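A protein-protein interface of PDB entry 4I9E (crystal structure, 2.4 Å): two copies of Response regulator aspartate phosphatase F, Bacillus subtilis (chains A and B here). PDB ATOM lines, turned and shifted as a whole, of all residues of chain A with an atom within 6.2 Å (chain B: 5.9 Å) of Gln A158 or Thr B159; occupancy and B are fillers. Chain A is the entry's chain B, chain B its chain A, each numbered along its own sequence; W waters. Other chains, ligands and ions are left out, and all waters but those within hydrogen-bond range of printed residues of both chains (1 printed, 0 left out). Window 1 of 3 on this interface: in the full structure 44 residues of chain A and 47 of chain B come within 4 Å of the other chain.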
ATOM      1  N   LEU A 120     -24.381  -3.758 -17.267  1.00  0.00           N
ATOM      2  CA  LEU A 120     -25.558  -3.382 -16.516  1.00  0.00           C
ATOM      3  C   LEU A 120     -26.431  -2.464 -17.312  1.00  0.00           C
ATOM      4  O   LEU A 120     -27.678  -2.528 -17.198  1.00  0.00           O
ATOM      5  CB  LEU A 120     -25.164  -2.682 -15.198  1.00  0.00           C
ATOM      6  CG  LEU A 120     -24.457  -3.552 -14.169  1.00  0.00           C
ATOM      7  CD1 LEU A 120     -24.369  -2.801 -12.845  1.00  0.00           C
ATOM      8  CD2 LEU A 120     -25.210  -4.898 -13.995  1.00  0.00           C
ATOM      9  N   ILE A 123     -28.209  -4.495 -19.949  1.00  0.00           N
ATOM     10  CA  ILE A 123     -29.382  -5.143 -19.313  1.00  0.00           C
ATOM     11  C   ILE A 123     -30.541  -4.166 -19.054  1.00  0.00           C
ATOM     12  O   ILE A 123     -31.712  -4.494 -19.269  1.00  0.00           O
ATOM     13  CB  ILE A 123     -28.983  -5.870 -18.033  1.00  0.00           C
ATOM     14  CG1 ILE A 123     -27.962  -6.948 -18.404  1.00  0.00           C
ATOM     15  CG2 ILE A 123     -30.206  -6.438 -17.299  1.00  0.00           C
ATOM     16  CD1 ILE A 123     -27.521  -7.831 -17.237  1.00  0.00           C
ATOM     17  N   TYR A 153     -26.754 -13.148 -23.247  1.00  0.00           N
ATOM     18  CA  TYR A 153     -26.504 -13.569 -21.868  1.00  0.00           C
ATOM     19  C   TYR A 153     -25.553 -14.766 -21.842  1.00  0.00           C
ATOM     20  O   TYR A 153     -24.945 -15.047 -20.819  1.00  0.00           O
ATOM     21  CB  TYR A 153     -27.840 -13.843 -21.166  1.00  0.00           C
ATOM     22  CG  TYR A 153     -28.618 -12.568 -20.984  1.00  0.00           C
ATOM     23  CD1 TYR A 153     -28.012 -11.461 -20.336  1.00  0.00           C
ATOM     24  CD2 TYR A 153     -29.930 -12.433 -21.450  1.00  0.00           C
ATOM     25  CE1 TYR A 153     -28.660 -10.261 -20.180  1.00  0.00           C
ATOM     26  CE2 TYR A 153     -30.612 -11.216 -21.270  1.00  0.00           C
ATOM     27  CZ  TYR A 153     -29.932 -10.123 -20.635  1.00  0.00           C
ATOM     28  OH  TYR A 153     -30.512  -8.899 -20.423  1.00  0.00           O
ATOM     29  N   TYR A 154     -25.444 -15.457 -22.975  1.00  0.00           N
ATOM     30  CA  TYR A 154     -24.411 -16.425 -23.202  1.00  0.00           C
ATOM     31  C   TYR A 154     -23.081 -15.685 -23.253  1.00  0.00           C
ATOM     32  O   TYR A 154     -22.165 -16.031 -22.532  1.00  0.00           O
ATOM     33  CB  TYR A 154     -24.625 -17.289 -24.493  1.00  0.00           C
ATOM     34  CG  TYR A 154     -23.401 -18.098 -24.775  1.00  0.00           C
ATOM     35  CD1 TYR A 154     -23.071 -19.183 -23.976  1.00  0.00           C
ATOM     36  CD2 TYR A 154     -22.513 -17.748 -25.831  1.00  0.00           C
ATOM     37  CE1 TYR A 154     -21.855 -19.913 -24.169  1.00  0.00           C
ATOM     38  CE2 TYR A 154     -21.319 -18.501 -26.068  1.00  0.00           C
ATOM     39  CZ  TYR A 154     -20.995 -19.570 -25.215  1.00  0.00           C
ATOM     40  OH  TYR A 154     -19.823 -20.324 -25.433  1.00  0.00           O
ATOM     41  N   TYR A 155     -22.984 -14.670 -24.103  1.00  0.00           N
ATOM     42  CA  TYR A 155     -21.803 -13.835 -24.147  1.00  0.00           C
ATOM     43  C   TYR A 155     -21.443 -13.223 -22.763  1.00  0.00           C
ATOM     44  O   TYR A 155     -20.272 -13.030 -22.472  1.00  0.00           O
ATOM     45  CB  TYR A 155     -21.959 -12.752 -25.219  1.00  0.00           C
ATOM     46  CG  TYR A 155     -22.193 -13.279 -26.629  1.00  0.00           C
ATOM     47  CD1 TYR A 155     -21.551 -14.430 -27.097  1.00  0.00           C
ATOM     48  CD2 TYR A 155     -23.014 -12.586 -27.515  1.00  0.00           C
ATOM     49  CE1 TYR A 155     -21.760 -14.893 -28.378  1.00  0.00           C
ATOM     50  CE2 TYR A 155     -23.218 -13.034 -28.806  1.00  0.00           C
ATOM     51  CZ  TYR A 155     -22.596 -14.191 -29.235  1.00  0.00           C
ATOM     52  OH  TYR A 155     -22.811 -14.613 -30.553  1.00  0.00           O
ATOM     53  N   MET A 156     -22.444 -12.937 -21.926  1.00  0.00           N
ATOM     54  CA  MET A 156     -22.251 -12.321 -20.581  1.00  0.00           C
ATOM     55  C   MET A 156     -22.119 -13.362 -19.468  1.00  0.00           C
ATOM     56  O   MET A 156     -22.007 -13.051 -18.251  1.00  0.00           O
ATOM     57  CB  MET A 156     -23.443 -11.414 -20.293  1.00  0.00           C
ATOM     58  CG  MET A 156     -23.321  -9.958 -20.867  1.00  0.00           C
ATOM     59  SD  MET A 156     -24.744  -8.863 -20.702  1.00  0.00           S
ATOM     60  CE  MET A 156     -24.907  -8.803 -18.962  1.00  0.00           C
ATOM     61  N   LYS A 157     -22.112 -14.634 -19.884  1.00  0.00           N
ATOM     62  CA  LYS A 157     -22.095 -15.804 -18.993  1.00  0.00           C
ATOM     63  C   LYS A 157     -23.125 -15.785 -17.881  1.00  0.00           C
ATOM     64  O   LYS A 157     -22.853 -16.246 -16.770  1.00  0.00           O
ATOM     65  CB  LYS A 157     -20.693 -16.039 -18.427  1.00  0.00           C
ATOM     66  CG  LYS A 157     -19.577 -16.320 -19.508  1.00  0.00           C
ATOM     67  CD  LYS A 157     -20.005 -17.378 -20.546  1.00  0.00           C
ATOM     68  CE  LYS A 157     -18.783 -17.882 -21.357  1.00  0.00           C
ATOM     69  NZ  LYS A 157     -19.075 -18.950 -22.376  1.00  0.00           N
ATOM     70  N   GLN A 158     -24.304 -15.219 -18.148  1.00  0.00           N
ATOM     71  CA  GLN A 158     -25.402 -15.265 -17.182  1.00  0.00           C
ATOM     72  C   GLN A 158     -26.132 -16.534 -17.659  1.00  0.00           C
ATOM     73  O   GLN A 158     -27.199 -16.442 -18.279  1.00  0.00           O
ATOM     74  CB  GLN A 158     -26.295 -14.007 -17.292  1.00  0.00           C
ATOM     75  CG  GLN A 158     -25.660 -12.635 -16.939  1.00  0.00           C
ATOM     76  CD  GLN A 158     -24.855 -12.637 -15.610  1.00  0.00           C
ATOM     77  OE1 GLN A 158     -23.685 -12.967 -15.572  1.00  0.00           O
ATOM     78  NE2 GLN A 158     -25.500 -12.335 -14.554  1.00  0.00           N
ATOM     79  N   THR A 159     -25.460 -17.691 -17.460  1.00  0.00           N
ATOM     80  CA  THR A 159     -25.824 -19.004 -18.022  1.00  0.00           C
ATOM     81  C   THR A 159     -27.284 -19.432 -17.818  1.00  0.00           C
ATOM     82  O   THR A 159     -27.920 -19.916 -18.765  1.00  0.00           O
ATOM     83  CB  THR A 159     -24.945 -20.079 -17.442  1.00  0.00           C
ATOM     84  OG1 THR A 159     -23.595 -19.623 -17.579  1.00  0.00           O
ATOM     85  CG2 THR A 159     -25.154 -21.422 -18.243  1.00  0.00           C
ATOM     86  N   TYR A 160     -27.831 -19.192 -16.634  1.00  0.00           N
ATOM     87  CA  TYR A 160     -29.166 -19.670 -16.383  1.00  0.00           C
ATOM     88  C   TYR A 160     -30.165 -18.850 -17.202  1.00  0.00           C
ATOM     89  O   TYR A 160     -31.068 -19.424 -17.837  1.00  0.00           O
ATOM     90  CB  TYR A 160     -29.502 -19.586 -14.894  1.00  0.00           C
ATOM     91  CG  TYR A 160     -28.622 -20.458 -14.026  1.00  0.00           C
ATOM     92  CD1 TYR A 160     -27.949 -21.533 -14.569  1.00  0.00           C
ATOM     93  CD2 TYR A 160     -28.490 -20.231 -12.654  1.00  0.00           C
ATOM     94  CE1 TYR A 160     -27.154 -22.320 -13.800  1.00  0.00           C
ATOM     95  CE2 TYR A 160     -27.664 -21.031 -11.874  1.00  0.00           C
ATOM     96  CZ  TYR A 160     -27.031 -22.076 -12.454  1.00  0.00           C
ATOM     97  OH  TYR A 160     -26.250 -22.944 -11.735  1.00  0.00           O
ATOM     98  N   PHE A 161     -30.032 -17.514 -17.167  1.00  0.00           N
ATOM     99  CA  PHE A 161     -30.883 -16.631 -17.899  1.00  0.00           C
ATOM    100  C   PHE A 161     -30.722 -16.892 -19.379  1.00  0.00           C
ATOM    101  O   PHE A 161     -31.689 -16.945 -20.144  1.00  0.00           O
ATOM    102  CB  PHE A 161     -30.506 -15.199 -17.543  1.00  0.00           C
ATOM    103  CG  PHE A 161     -31.179 -14.703 -16.290  1.00  0.00           C
ATOM    104  CD1 PHE A 161     -32.460 -14.177 -16.334  1.00  0.00           C
ATOM    105  CD2 PHE A 161     -30.538 -14.794 -15.071  1.00  0.00           C
ATOM    106  CE1 PHE A 161     -33.074 -13.729 -15.165  1.00  0.00           C
ATOM    107  CE2 PHE A 161     -31.163 -14.407 -13.934  1.00  0.00           C
ATOM    108  CZ  PHE A 161     -32.445 -13.831 -13.975  1.00  0.00           C
ATOM    109  N   SER A 162     -29.510 -17.124 -19.828  1.00  0.00           N
ATOM    110  CA  SER A 162     -29.338 -17.529 -21.224  1.00  0.00           C
ATOM    111  C   SER A 162     -30.130 -18.793 -21.642  1.00  0.00           C
ATOM    112  O   SER A 162     -30.623 -18.884 -22.772  1.00  0.00           O
ATOM    113  CB  SER A 162     -27.892 -17.683 -21.519  1.00  0.00           C
ATOM    114  OG  SER A 162     -27.750 -18.140 -22.846  1.00  0.00           O
ATOM    115  N   MET A 163     -30.190 -19.784 -20.757  1.00  0.00           N
ATOM    116  CA  MET A 163     -30.912 -21.014 -20.983  1.00  0.00           C
ATOM    117  C   MET A 163     -32.419 -20.789 -20.878  1.00  0.00           C
ATOM    118  O   MET A 163     -33.156 -21.248 -21.733  1.00  0.00           O
ATOM    119  CB  MET A 163     -30.463 -22.047 -19.966  1.00  0.00           C
ATOM    120  CG  MET A 163     -29.140 -22.639 -20.447  1.00  0.00           C
ATOM    121  SD  MET A 163     -28.498 -23.901 -19.367  1.00  0.00           S
ATOM    122  CE  MET A 163     -28.844 -25.310 -20.381  1.00  0.00           C
ATOM    123  N   ASN A 193     -24.341 -23.577 -23.291  1.00  0.00           N
ATOM    124  CA  ASN A 193     -24.546 -23.295 -21.878  1.00  0.00           C
ATOM    125  C   ASN A 193     -24.275 -24.479 -20.972  1.00  0.00           C
ATOM    126  O   ASN A 193     -23.677 -24.306 -19.946  1.00  0.00           O
ATOM    127  CB  ASN A 193     -25.968 -22.801 -21.685  1.00  0.00           C
ATOM    128  CG  ASN A 193     -26.156 -21.336 -22.130  1.00  0.00           C
ATOM    129  OD1 ASN A 193     -25.545 -20.434 -21.560  1.00  0.00           O
ATOM    130  ND2 ASN A 193     -26.994 -21.109 -23.152  1.00  0.00           N
ATOM    131  N   TYR B 153     -30.477 -14.190  -7.191  1.00  0.00           N
ATOM    132  CA  TYR B 153     -29.527 -14.196  -8.327  1.00  0.00           C
ATOM    133  C   TYR B 153     -28.077 -14.037  -7.878  1.00  0.00           C
ATOM    134  O   TYR B 153     -27.140 -14.433  -8.581  1.00  0.00           O
ATOM    135  CB  TYR B 153     -29.993 -13.211  -9.384  1.00  0.00           C
ATOM    136  CG  TYR B 153     -31.318 -13.682  -9.995  1.00  0.00           C
ATOM    137  CD1 TYR B 153     -31.446 -14.977 -10.555  1.00  0.00           C
ATOM    138  CD2 TYR B 153     -32.453 -12.866  -9.978  1.00  0.00           C
ATOM    139  CE1 TYR B 153     -32.655 -15.427 -11.066  1.00  0.00           C
ATOM    140  CE2 TYR B 153     -33.656 -13.305 -10.493  1.00  0.00           C
ATOM    141  CZ  TYR B 153     -33.747 -14.581 -11.036  1.00  0.00           C
ATOM    142  OH  TYR B 153     -34.930 -14.969 -11.574  1.00  0.00           O
ATOM    143  N   MET B 156     -27.351 -17.622  -7.097  1.00  0.00           N
ATOM    144  CA  MET B 156     -27.176 -18.362  -8.376  1.00  0.00           C
ATOM    145  C   MET B 156     -25.971 -17.858  -9.211  1.00  0.00           C
ATOM    146  O   MET B 156     -25.690 -18.374 -10.324  1.00  0.00           O
ATOM    147  CB  MET B 156     -28.466 -18.291  -9.187  1.00  0.00           C
ATOM    148  CG  MET B 156     -29.668 -19.011  -8.574  1.00  0.00           C
ATOM    149  SD  MET B 156     -31.280 -18.916  -9.459  1.00  0.00           S
ATOM    150  CE  MET B 156     -30.833 -19.376 -11.054  1.00  0.00           C
ATOM    151  N   LYS B 157     -25.303 -16.806  -8.709  1.00  0.00           N
ATOM    152  CA  LYS B 157     -24.167 -16.131  -9.355  1.00  0.00           C
ATOM    153  C   LYS B 157     -24.499 -15.573 -10.746  1.00  0.00           C
ATOM    154  O   LYS B 157     -23.654 -15.532 -11.664  1.00  0.00           O
ATOM    155  CB  LYS B 157     -22.902 -16.999  -9.377  1.00  0.00           C
ATOM    156  CG  LYS B 157     -22.343 -17.388  -7.959  1.00  0.00           C
ATOM    157  CD  LYS B 157     -22.171 -16.136  -7.125  1.00  0.00           C
ATOM    158  CE  LYS B 157     -21.565 -16.357  -5.737  1.00  0.00           C
ATOM    159  NZ  LYS B 157     -22.794 -16.334  -4.827  1.00  0.00           N
ATOM    160  N   GLN B 158     -25.746 -15.119 -10.913  1.00  0.00           N
ATOM    161  CA  GLN B 158     -26.132 -14.458 -12.139  1.00  0.00           C
ATOM    162  C   GLN B 158     -25.888 -13.008 -11.718  1.00  0.00           C
ATOM    163  O   GLN B 158     -26.837 -12.285 -11.523  1.00  0.00           O
ATOM    164  CB  GLN B 158     -27.589 -14.772 -12.489  1.00  0.00           C
ATOM    165  CG  GLN B 158     -27.879 -16.307 -12.649  1.00  0.00           C
ATOM    166  CD  GLN B 158     -26.983 -16.993 -13.699  1.00  0.00           C
ATOM    167  OE1 GLN B 158     -25.948 -17.534 -13.367  1.00  0.00           O
ATOM    168  NE2 GLN B 158     -27.348 -16.942 -14.923  1.00  0.00           N
ATOM    169  N   THR B 159     -24.597 -12.654 -11.522  1.00  0.00           N
ATOM    170  CA  THR B 159     -24.109 -11.337 -11.009  1.00  0.00           C
ATOM    171  C   THR B 159     -24.774 -10.097 -11.616  1.00  0.00           C
ATOM    172  O   THR B 159     -25.256  -9.266 -10.877  1.00  0.00           O
ATOM    173  CB  THR B 159     -22.550 -11.288 -11.108  1.00  0.00           C
ATOM    174  OG1 THR B 159     -22.072 -12.504 -10.540  1.00  0.00           O
ATOM    175  CG2 THR B 159     -21.919 -10.198 -10.223  1.00  0.00           C
ATOM    176  N   TYR B 160     -24.831  -9.999 -12.948  1.00  0.00           N
ATOM    177  CA  TYR B 160     -25.386  -8.869 -13.578  1.00  0.00           C
ATOM    178  C   TYR B 160     -26.856  -8.678 -13.251  1.00  0.00           C
ATOM    179  O   TYR B 160     -27.274  -7.572 -12.923  1.00  0.00           O
ATOM    180  CB  TYR B 160     -25.134  -8.900 -15.089  1.00  0.00           C
ATOM    181  CG  TYR B 160     -23.665  -8.934 -15.433  1.00  0.00           C
ATOM    182  CD1 TYR B 160     -22.710  -8.546 -14.520  1.00  0.00           C
ATOM    183  CD2 TYR B 160     -23.230  -9.404 -16.675  1.00  0.00           C
ATOM    184  CE1 TYR B 160     -21.352  -8.646 -14.846  1.00  0.00           C
ATOM    185  CE2 TYR B 160     -21.905  -9.480 -16.991  1.00  0.00           C
ATOM    186  CZ  TYR B 160     -20.971  -9.098 -16.085  1.00  0.00           C
ATOM    187  OH  TYR B 160     -19.626  -9.141 -16.440  1.00  0.00           O
ATOM    188  N   PHE B 161     -27.659  -9.760 -13.308  1.00  0.00           N
ATOM    189  CA  PHE B 161     -29.075  -9.657 -12.915  1.00  0.00           C
ATOM    190  C   PHE B 161     -29.203  -9.389 -11.441  1.00  0.00           C
ATOM    191  O   PHE B 161     -30.104  -8.683 -11.051  1.00  0.00           O
ATOM    192  CB  PHE B 161     -29.862 -10.899 -13.319  1.00  0.00           C
ATOM    193  CG  PHE B 161     -30.031 -11.050 -14.792  1.00  0.00           C
ATOM    194  CD1 PHE B 161     -31.175 -10.558 -15.428  1.00  0.00           C
ATOM    195  CD2 PHE B 161     -29.061 -11.670 -15.546  1.00  0.00           C
ATOM    196  CE1 PHE B 161     -31.345 -10.739 -16.806  1.00  0.00           C
ATOM    197  CE2 PHE B 161     -29.231 -11.802 -16.885  1.00  0.00           C
ATOM    198  CZ  PHE B 161     -30.368 -11.345 -17.535  1.00  0.00           C
ATOM    199  N   SER B 162     -28.345  -9.949 -10.598  1.00  0.00           N
ATOM    200  CA  SER B 162     -28.442  -9.639  -9.152  1.00  0.00           C
ATOM    201  C   SER B 162     -28.252  -8.143  -8.904  1.00  0.00           C
ATOM    202  O   SER B 162     -28.981  -7.566  -8.105  1.00  0.00           O
ATOM    203  CB  SER B 162     -27.402 -10.400  -8.346  1.00  0.00           C
ATOM    204  OG  SER B 162     -27.497 -10.078  -6.937  1.00  0.00           O
ATOM    205  N   MET B 163     -27.275  -7.509  -9.576  1.00  0.00           N
ATOM    206  CA  MET B 163     -27.093  -6.057  -9.473  1.00  0.00           C
ATOM    207  C   MET B 163     -28.174  -5.194 -10.125  1.00  0.00           C
ATOM    208  O   MET B 163     -28.612  -4.174  -9.547  1.00  0.00           O
ATOM    209  CB  MET B 163     -25.723  -5.668 -10.024  1.00  0.00           C
ATOM    210  CG  MET B 163     -24.609  -6.243  -9.186  1.00  0.00           C
ATOM    211  SD  MET B 163     -23.038  -6.047  -9.963  1.00  0.00           S
ATOM    212  CE  MET B 163     -22.647  -4.569  -8.972  1.00  0.00           C
ATOM    213  N   ASP B 164     -28.586  -5.525 -11.345  1.00  0.00           N
ATOM    214  CA  ASP B 164     -29.756  -4.901 -11.883  1.00  0.00           C
ATOM    215  C   ASP B 164     -30.996  -4.941 -10.967  1.00  0.00           C
ATOM    216  O   ASP B 164     -31.681  -3.920 -10.811  1.00  0.00           O
ATOM    217  CB  ASP B 164     -30.129  -5.583 -13.174  1.00  0.00           C
ATOM    218  CG  ASP B 164     -31.299  -4.923 -13.827  1.00  0.00           C
ATOM    219  OD1 ASP B 164     -31.123  -3.817 -14.345  1.00  0.00           O
ATOM    220  OD2 ASP B 164     -32.372  -5.498 -13.813  1.00  0.00           O
ATOM    221  N   ASN B 193     -21.714  -8.635  -5.026  1.00  0.00           N
ATOM    222  CA  ASN B 193     -21.596  -8.903  -6.456  1.00  0.00           C
ATOM    223  C   ASN B 193     -20.305  -8.298  -7.016  1.00  0.00           C
ATOM    224  O   ASN B 193     -19.620  -8.925  -7.816  1.00  0.00           O
ATOM    225  CB  ASN B 193     -22.851  -8.355  -7.178  1.00  0.00           C
ATOM    226  CG  ASN B 193     -24.093  -9.188  -6.924  1.00  0.00           C
ATOM    227  OD1 ASN B 193     -25.099  -8.734  -6.301  1.00  0.00           O
ATOM    228  ND2 ASN B 193     -24.049 -10.408  -7.390  1.00  0.00           N
ATOM    229  N   PHE B 194     -19.946  -7.065  -6.615  1.00  0.00           N
ATOM    230  CA  PHE B 194     -18.642  -6.489  -7.044  1.00  0.00           C
ATOM    231  C   PHE B 194     -17.482  -7.441  -6.720  1.00  0.00           C
ATOM    232  O   PHE B 194     -16.547  -7.561  -7.515  1.00  0.00           O
ATOM    233  CB  PHE B 194     -18.361  -5.129  -6.396  1.00  0.00           C
ATOM    234  CG  PHE B 194     -18.956  -3.957  -7.137  1.00  0.00           C
ATOM    235  CD1 PHE B 194     -18.720  -3.770  -8.524  1.00  0.00           C
ATOM    236  CD2 PHE B 194     -19.705  -2.999  -6.450  1.00  0.00           C
ATOM    237  CE1 PHE B 194     -19.243  -2.696  -9.182  1.00  0.00           C
ATOM    238  CE2 PHE B 194     -20.231  -1.912  -7.143  1.00  0.00           C
ATOM    239  CZ  PHE B 194     -19.990  -1.767  -8.497  1.00  0.00           C
ATOM    240  N   ASP B 196     -17.498 -10.767  -6.327  1.00  0.00           N
ATOM    241  CA  ASP B 196     -17.500 -11.886  -7.277  1.00  0.00           C
ATOM    242  C   ASP B 196     -16.924 -11.584  -8.638  1.00  0.00           C
ATOM    243  O   ASP B 196     -16.522 -12.484  -9.357  1.00  0.00           O
ATOM    244  CB  ASP B 196     -18.880 -12.451  -7.489  1.00  0.00           C
ATOM    245  CG  ASP B 196     -19.414 -13.179  -6.277  1.00  0.00           C
ATOM    246  OD1 ASP B 196     -18.634 -13.464  -5.331  1.00  0.00           O
ATOM    247  OD2 ASP B 196     -20.658 -13.433  -6.278  1.00  0.00           O
ATOM    248  N   LEU B 197     -16.913 -10.311  -9.002  1.00  0.00           N
ATOM    249  CA  LEU B 197     -16.343  -9.855 -10.268  1.00  0.00           C
ATOM    250  C   LEU B 197     -14.910  -9.435 -10.126  1.00  0.00           C
ATOM    251  O   LEU B 197     -14.286  -9.097 -11.135  1.00  0.00           O
ATOM    252  CB  LEU B 197     -17.125  -8.693 -10.803  1.00  0.00           C
ATOM    253  CG  LEU B 197     -18.595  -8.958 -11.153  1.00  0.00           C
ATOM    254  CD1 LEU B 197     -19.240  -7.620 -11.549  1.00  0.00           C
ATOM    255  CD2 LEU B 197     -18.847 -10.046 -12.207  1.00  0.00           C
HETATM  256  O   HOH W   1     -28.616  -2.645 -14.790  1.00  0.00           O
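N of Thr B159 lies close to NE2 of Gln A158, at 3.2 Å. O of Gln B158 sits close to NE2 of Gln A158, at 3.3 Å. N of Tyr A160 lies close to NE2 of Gln B158, at 2.9 Å. NE2 of Gln B158 sits close to N of Thr A159. N of Tyr B160 sits close to NE2 of Gln A158 (2.9 Å).
O of Tyr B153 lies within hydrogen-bond range of N of Gln B158 (2.8 Å). O of Met B156 sits close to OE1 of Gln B158 (3.2 Å). The backbone carbonyl oxygen (O) of Tyr A153 is in hydrogen-bond range of the backbone NH (N) of Gln A158, at 2.8 Å. The backbone carbonyl oxygen of Met A156 sits close to the side-chain amide oxygen of Gln A158 (3.2 Å).
Among the printed residues, merely in contact across the chains: Met A156 with Tyr B160 (2.9 Å), Tyr A160 with Met B156 (3.0 Å), Phe A161 with Tyr B153 (3.3 Å), Tyr A153 with Phe B161 (3.3 Å), Ile A123 with Tyr B160 (3.4 Å), Phe A161 with Phe B161 (3.5 Å), Leu A120 with Tyr B160 (3.5 Å), Phe A161 with Gln B158 (3.5 Å), Gln A158 with Phe B161 (3.6 Å) and Ile A123 with Asp B164 (3.9 Å).
Of chain B, only Gln B158, Thr B159, Tyr B160 and Phe B161 come within 4 Å of Gln A158. Of the printed residues of chain B, Tyr A153 touches Phe B161 (3.3 Å). Of the printed residues of chain A, Asp B164 touches Ile A123. Of the printed residues of chain B, Met A156 touches Tyr B160. Of the printed residues of chain B, Phe A161 touches Tyr B153, Gln B158 and Phe B161. The nearest residue of chain B that does not touch Gln A158 is Lys B157 (4.7 Å). The nearest residue of chain A that does not touch Thr B159 is Leu A120 (5.4 Å). The nearest printed residue of chain B that does not touch Phe A161 is Met B156 (5.8 Å).
Printed residues of chain B that touch a printed residue of chain A: Tyr B153, Met B156, Gln B158, Thr B159, Tyr B160, Phe B161 and Asp B164. Hydrophobic or aromatic side chains of chain B within 4 Å of the printed part of chain A: Tyr B153, Met B156, Tyr B160 and Phe B161. Among the printed residues, no Asp or Glu carboxylate lies within 4 Å of a Lys or Arg side-chain nitrogen of the other chain.
Tyr A153 touches Phe B161, and with the chains exchanged Phe A161 touches Tyr B153. Gln A158 touches Thr B159, and with the chains exchanged Thr A159 touches Gln B158. Gln A158 touches Phe B161, and with the chains exchanged Phe A161 touches Gln B158. Phe A161 touches its own counterpart, Phe B161. Of the 15 pairs that touch across the chains among the printed residues, 12 have their exchanged pair printed and touching as well.
Water W1 bridges the backbone carbonyl oxygen of Leu A120 (2.6 Å) and the side-chain carboxylate of Asp B164 (2.8 Å).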
